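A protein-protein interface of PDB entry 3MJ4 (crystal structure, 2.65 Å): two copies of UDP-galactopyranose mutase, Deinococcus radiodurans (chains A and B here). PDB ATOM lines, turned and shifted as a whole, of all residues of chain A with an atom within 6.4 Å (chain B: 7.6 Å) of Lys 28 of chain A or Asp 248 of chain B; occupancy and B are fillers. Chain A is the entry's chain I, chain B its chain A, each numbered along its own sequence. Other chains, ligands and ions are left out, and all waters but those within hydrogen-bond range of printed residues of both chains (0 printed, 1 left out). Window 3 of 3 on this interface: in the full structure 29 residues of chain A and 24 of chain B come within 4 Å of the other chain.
Position printed for both chains: 251.
Of the 8 pairs that touch across the chains among the printed residues, none has its exchanged pair printed and touching as well.
Among the printed residues, pairs that only touch across the chains: Ser 27 of chain A with Phe 249 of chain B (3.4 Å), Lys 28 of chain A with Phe 249 of chain B (3.4 Å), Gly 29 of chain A with Phe 249 of chain B (3.4 Å), Pro 251 of chain A with Phe 249 of chain B (3.6 Å), Phe 30 of chain A with Phe 249 of chain B (3.7 Å) and Glu 26 of chain A with Asp 248 of chain B (3.7 Å).
Printed residues of chain B within 4 Å of Lys 28 of chain A: Asp 248 (2.7 Å) and Phe 249 (3.4 Å).
Printed residues of chain B within 4 Å of Phe 30 of chain A: Phe 249 (3.7 Å).
Printed residues of chain A within 4 Å of Arg 244 of chain B: Glu 26.
Printed residues of chain A within 4 Å of Asp 248 of chain B: Glu 26 (3.7 Å) and Lys 28 (2.7 Å).
The nearest printed residue of chain A that does not touch Asp 248 of chain B is Ser 27 of chain A (4.0004 Å).
The nearest printed residue of chain B that does not touch Ser 27 of chain A is Asp 248 of chain B (4.0004 Å).
The side-chain carboxylate (OD2) of Asp 248 of chain B is in salt-bridge range of the side-chain amino group (NZ) of Lys 28 of chain A (2.7 Å).
O of Arg 244 of chain B lies within hydrogen-bond range of N of Glu 26 of chain A.
Hydrophobic or aromatic side chains of chain A that line the printed part of chain B: Phe 30 and Pro 251.
Along chain A the printed residues that touch a printed residue of chain B span positions 26 to 251.
Of the 10 printed residues of chain B, 3 touch a printed residue of chain A.
Hydrophobic or aromatic side chains of chain B within 4 Å of the printed part of chain A: Phe 249.
Among the printed residues, 8 pairs touch across the chains.
The backbone NH of Phe 30 of chain A is in hydrogen-bond range of the backbone carbonyl oxygen of Pro 251 of chain A, at 2.7 Å.
The backbone carbonyl oxygen of Glu 26 of chain A lies within hydrogen-bond range of the side-chain amino group of Lys 28 of chain A (3.2 Å).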
ATOM      1  N   GLU A  26      -9.715  -7.042  16.062  1.00  0.00           N
ATOM      2  CA  GLU A  26     -11.140  -6.965  16.386  1.00  0.00           C
ATOM      3  C   GLU A  26     -11.483  -7.335  17.842  1.00  0.00           C
ATOM      4  O   GLU A  26     -12.376  -6.726  18.447  1.00  0.00           O
ATOM      5  CB  GLU A  26     -11.965  -7.837  15.421  1.00  0.00           C
ATOM      6  CG  GLU A  26     -13.481  -7.709  15.582  1.00  0.00           C
ATOM      7  CD  GLU A  26     -13.992  -6.305  15.260  1.00  0.00           C
ATOM      8  OE1 GLU A  26     -14.892  -6.192  14.396  1.00  0.00           O
ATOM      9  OE2 GLU A  26     -13.498  -5.320  15.869  1.00  0.00           O
ATOM     10  N   SER A  27     -10.785  -8.331  18.393  1.00  0.00           N
ATOM     11  CA  SER A  27     -11.146  -8.902  19.699  1.00  0.00           C
ATOM     12  C   SER A  27     -10.979  -7.905  20.857  1.00  0.00           C
ATOM     13  O   SER A  27     -10.178  -6.973  20.785  1.00  0.00           O
ATOM     14  CB  SER A  27     -10.367 -10.198  19.961  1.00  0.00           C
ATOM     15  OG  SER A  27     -11.076 -11.057  20.845  1.00  0.00           O
ATOM     16  N   LYS A  28     -11.742  -8.109  21.926  1.00  0.00           N
ATOM     17  CA  LYS A  28     -11.860  -7.094  22.973  1.00  0.00           C
ATOM     18  C   LYS A  28     -11.297  -7.566  24.314  1.00  0.00           C
ATOM     19  O   LYS A  28     -11.380  -6.860  25.321  1.00  0.00           O
ATOM     20  CB  LYS A  28     -13.322  -6.665  23.117  1.00  0.00           C
ATOM     21  CG  LYS A  28     -13.508  -5.185  23.380  1.00  0.00           C
ATOM     22  CD  LYS A  28     -12.916  -4.352  22.256  1.00  0.00           C
ATOM     23  CE  LYS A  28     -13.573  -4.661  20.915  1.00  0.00           C
ATOM     24  NZ  LYS A  28     -12.914  -3.926  19.792  1.00  0.00           N
ATOM     25  N   GLY A  29     -10.711  -8.757  24.314  1.00  0.00           N
ATOM     26  CA  GLY A  29     -10.103  -9.318  25.510  1.00  0.00           C
ATOM     27  C   GLY A  29     -10.165 -10.831  25.455  1.00  0.00           C
ATOM     28  O   GLY A  29     -10.391 -11.414  24.380  1.00  0.00           O
ATOM     29  N   PHE A  30      -9.983 -11.467  26.614  1.00  0.00           N
ATOM     30  CA  PHE A  30      -9.891 -12.931  26.700  1.00  0.00           C
ATOM     31  C   PHE A  30     -10.914 -13.541  27.648  1.00  0.00           C
ATOM     32  O   PHE A  30     -11.371 -12.900  28.602  1.00  0.00           O
ATOM     33  CB  PHE A  30      -8.505 -13.367  27.197  1.00  0.00           C
ATOM     34  CG  PHE A  30      -7.367 -12.871  26.371  1.00  0.00           C
ATOM     35  CD1 PHE A  30      -6.646 -11.755  26.766  1.00  0.00           C
ATOM     36  CD2 PHE A  30      -6.980 -13.549  25.224  1.00  0.00           C
ATOM     37  CE1 PHE A  30      -5.570 -11.307  26.014  1.00  0.00           C
ATOM     38  CE2 PHE A  30      -5.919 -13.114  24.465  1.00  0.00           C
ATOM     39  CZ  PHE A  30      -5.204 -11.992  24.858  1.00  0.00           C
ATOM     40  N   PRO A 251      -8.114  -7.607  29.871  1.00  0.00           N
ATOM     41  CA  PRO A 251      -9.445  -8.134  30.169  1.00  0.00           C
ATOM     42  C   PRO A 251      -9.544  -9.647  30.043  1.00  0.00           C
ATOM     43  O   PRO A 251      -9.377 -10.185  28.954  1.00  0.00           O
ATOM     44  CB  PRO A 251     -10.325  -7.472  29.101  1.00  0.00           C
ATOM     45  CG  PRO A 251      -9.629  -6.204  28.791  1.00  0.00           C
ATOM     46  CD  PRO A 251      -8.159  -6.501  28.897  1.00  0.00           C
ATOM     47  N   TYR B 243      -0.983  -7.962  15.927  1.00  0.00           N
ATOM     48  CA  TYR B 243      -1.122  -6.845  16.843  1.00  0.00           C
ATOM     49  C   TYR B 243      -2.577  -6.402  16.869  1.00  0.00           C
ATOM     50  O   TYR B 243      -3.111  -6.014  17.906  1.00  0.00           O
ATOM     51  CB  TYR B 243      -0.192  -5.691  16.479  1.00  0.00           C
ATOM     52  CG  TYR B 243      -0.593  -4.965  15.229  1.00  0.00           C
ATOM     53  CD1 TYR B 243      -1.339  -3.790  15.283  1.00  0.00           C
ATOM     54  CD2 TYR B 243      -0.233  -5.458  13.987  1.00  0.00           C
ATOM     55  CE1 TYR B 243      -1.713  -3.127  14.121  1.00  0.00           C
ATOM     56  CE2 TYR B 243      -0.592  -4.804  12.834  1.00  0.00           C
ATOM     57  CZ  TYR B 243      -1.332  -3.644  12.899  1.00  0.00           C
ATOM     58  OH  TYR B 243      -1.680  -3.020  11.722  1.00  0.00           O
ATOM     59  N   ARG B 244      -3.229  -6.501  15.723  1.00  0.00           N
ATOM     60  CA  ARG B 244      -4.611  -6.087  15.627  1.00  0.00           C
ATOM     61  C   ARG B 244      -5.498  -6.860  16.607  1.00  0.00           C
ATOM     62  O   ARG B 244      -6.472  -6.314  17.129  1.00  0.00           O
ATOM     63  CB  ARG B 244      -5.098  -6.189  14.179  1.00  0.00           C
ATOM     64  CG  ARG B 244      -4.601  -5.038  13.320  1.00  0.00           C
ATOM     65  CD  ARG B 244      -4.700  -5.346  11.838  1.00  0.00           C
ATOM     66  NE  ARG B 244      -4.039  -6.611  11.525  1.00  0.00           N
ATOM     67  CZ  ARG B 244      -3.771  -7.043  10.295  1.00  0.00           C
ATOM     68  NH1 ARG B 244      -4.096  -6.308   9.235  1.00  0.00           N
ATOM     69  NH2 ARG B 244      -3.173  -8.216  10.126  1.00  0.00           N
ATOM     70  N   GLU B 245      -5.136  -8.114  16.877  1.00  0.00           N
ATOM     71  CA  GLU B 245      -5.852  -8.921  17.866  1.00  0.00           C
ATOM     72  C   GLU B 245      -5.751  -8.374  19.298  1.00  0.00           C
ATOM     73  O   GLU B 245      -6.580  -8.731  20.134  1.00  0.00           O
ATOM     74  CB  GLU B 245      -5.363 -10.378  17.877  1.00  0.00           C
ATOM     75  CG  GLU B 245      -5.710 -11.216  16.659  1.00  0.00           C
ATOM     76  CD  GLU B 245      -5.119 -12.640  16.735  1.00  0.00           C
ATOM     77  OE1 GLU B 245      -3.893 -12.821  16.497  1.00  0.00           O
ATOM     78  OE2 GLU B 245      -5.884 -13.586  17.032  1.00  0.00           O
ATOM     79  N   ILE B 246      -4.749  -7.542  19.601  1.00  0.00           N
ATOM     80  CA  ILE B 246      -4.628  -7.008  20.965  1.00  0.00           C
ATOM     81  C   ILE B 246      -4.649  -5.493  21.079  1.00  0.00           C
ATOM     82  O   ILE B 246      -4.750  -4.963  22.188  1.00  0.00           O
ATOM     83  CB  ILE B 246      -3.316  -7.427  21.668  1.00  0.00           C
ATOM     84  CG1 ILE B 246      -2.124  -6.879  20.886  1.00  0.00           C
ATOM     85  CG2 ILE B 246      -3.254  -8.934  21.881  1.00  0.00           C
ATOM     86  CD1 ILE B 246      -0.839  -7.064  21.580  1.00  0.00           C
ATOM     87  N   ALA B 247      -4.536  -4.789  19.961  1.00  0.00           N
ATOM     88  CA  ALA B 247      -4.346  -3.342  20.024  1.00  0.00           C
ATOM     89  C   ALA B 247      -5.559  -2.545  20.542  1.00  0.00           C
ATOM     90  O   ALA B 247      -5.394  -1.411  20.990  1.00  0.00           O
ATOM     91  CB  ALA B 247      -3.849  -2.790  18.684  1.00  0.00           C
ATOM     92  N   ASP B 248      -6.759  -3.125  20.493  1.00  0.00           N
ATOM     93  CA  ASP B 248      -7.950  -2.427  21.002  1.00  0.00           C
ATOM     94  C   ASP B 248      -7.978  -2.355  22.512  1.00  0.00           C
ATOM     95  O   ASP B 248      -8.559  -1.429  23.069  1.00  0.00           O
ATOM     96  CB  ASP B 248      -9.256  -3.088  20.541  1.00  0.00           C
ATOM     97  CG  ASP B 248      -9.509  -2.916  19.056  1.00  0.00           C
ATOM     98  OD1 ASP B 248      -8.720  -2.195  18.393  1.00  0.00           O
ATOM     99  OD2 ASP B 248     -10.505  -3.502  18.562  1.00  0.00           O
ATOM    100  N   PHE B 249      -7.362  -3.334  23.173  1.00  0.00           N
ATOM    101  CA  PHE B 249      -7.448  -3.418  24.624  1.00  0.00           C
ATOM    102  C   PHE B 249      -6.128  -3.497  25.401  1.00  0.00           C
ATOM    103  O   PHE B 249      -6.145  -3.407  26.625  1.00  0.00           O
ATOM    104  CB  PHE B 249      -8.348  -4.576  25.031  1.00  0.00           C
ATOM    105  CG  PHE B 249      -7.813  -5.904  24.662  1.00  0.00           C
ATOM    106  CD1 PHE B 249      -8.159  -6.490  23.460  1.00  0.00           C
ATOM    107  CD2 PHE B 249      -6.945  -6.578  25.520  1.00  0.00           C
ATOM    108  CE1 PHE B 249      -7.658  -7.738  23.118  1.00  0.00           C
ATOM    109  CE2 PHE B 249      -6.431  -7.824  25.186  1.00  0.00           C
ATOM    110  CZ  PHE B 249      -6.794  -8.406  23.988  1.00  0.00           C
ATOM    111  N   ILE B 250      -4.990  -3.674  24.738  1.00  0.00           N
ATOM    112  CA  ILE B 250      -3.741  -3.526  25.488  1.00  0.00           C
ATOM    113  C   ILE B 250      -3.196  -2.114  25.372  1.00  0.00           C
ATOM    114  O   ILE B 250      -2.955  -1.630  24.278  1.00  0.00           O
ATOM    115  CB  ILE B 250      -2.660  -4.549  25.118  1.00  0.00           C
ATOM    116  CG1 ILE B 250      -3.154  -5.955  25.432  1.00  0.00           C
ATOM    117  CG2 ILE B 250      -1.412  -4.282  25.943  1.00  0.00           C
ATOM    118  CD1 ILE B 250      -2.257  -7.036  24.951  1.00  0.00           C
ATOM    119  N   PRO B 251      -3.031  -1.434  26.513  1.00  0.00           N
ATOM    120  CA  PRO B 251      -2.583  -0.038  26.523  1.00  0.00           C
ATOM    121  C   PRO B 251      -1.140   0.042  26.059  1.00  0.00           C
ATOM    122  O   PRO B 251      -0.329  -0.767  26.502  1.00  0.00           O
ATOM    123  CB  PRO B 251      -2.640   0.347  28.006  1.00  0.00           C
ATOM    124  CG  PRO B 251      -3.349  -0.741  28.687  1.00  0.00           C
ATOM    125  CD  PRO B 251      -3.192  -1.975  27.869  1.00  0.00           C
ATOM    126  N   PHE B 252      -0.828   0.992  25.186  1.00  0.00           N
ATOM    127  CA  PHE B 252       0.557   1.247  24.799  1.00  0.00           C
ATOM    128  C   PHE B 252       0.699   2.704  24.390  1.00  0.00           C
ATOM    129  O   PHE B 252      -0.243   3.289  23.886  1.00  0.00           O
ATOM    130  CB  PHE B 252       1.037   0.278  23.698  1.00  0.00           C
ATOM    131  CG  PHE B 252       0.295   0.396  22.408  1.00  0.00           C
ATOM    132  CD1 PHE B 252       0.750   1.245  21.406  1.00  0.00           C
ATOM    133  CD2 PHE B 252      -0.864  -0.341  22.188  1.00  0.00           C
ATOM    134  CE1 PHE B 252       0.053   1.374  20.176  1.00  0.00           C
ATOM    135  CE2 PHE B 252      -1.576  -0.221  20.985  1.00  0.00           C
ATOM    136  CZ  PHE B 252      -1.112   0.638  19.963  1.00  0.00           C
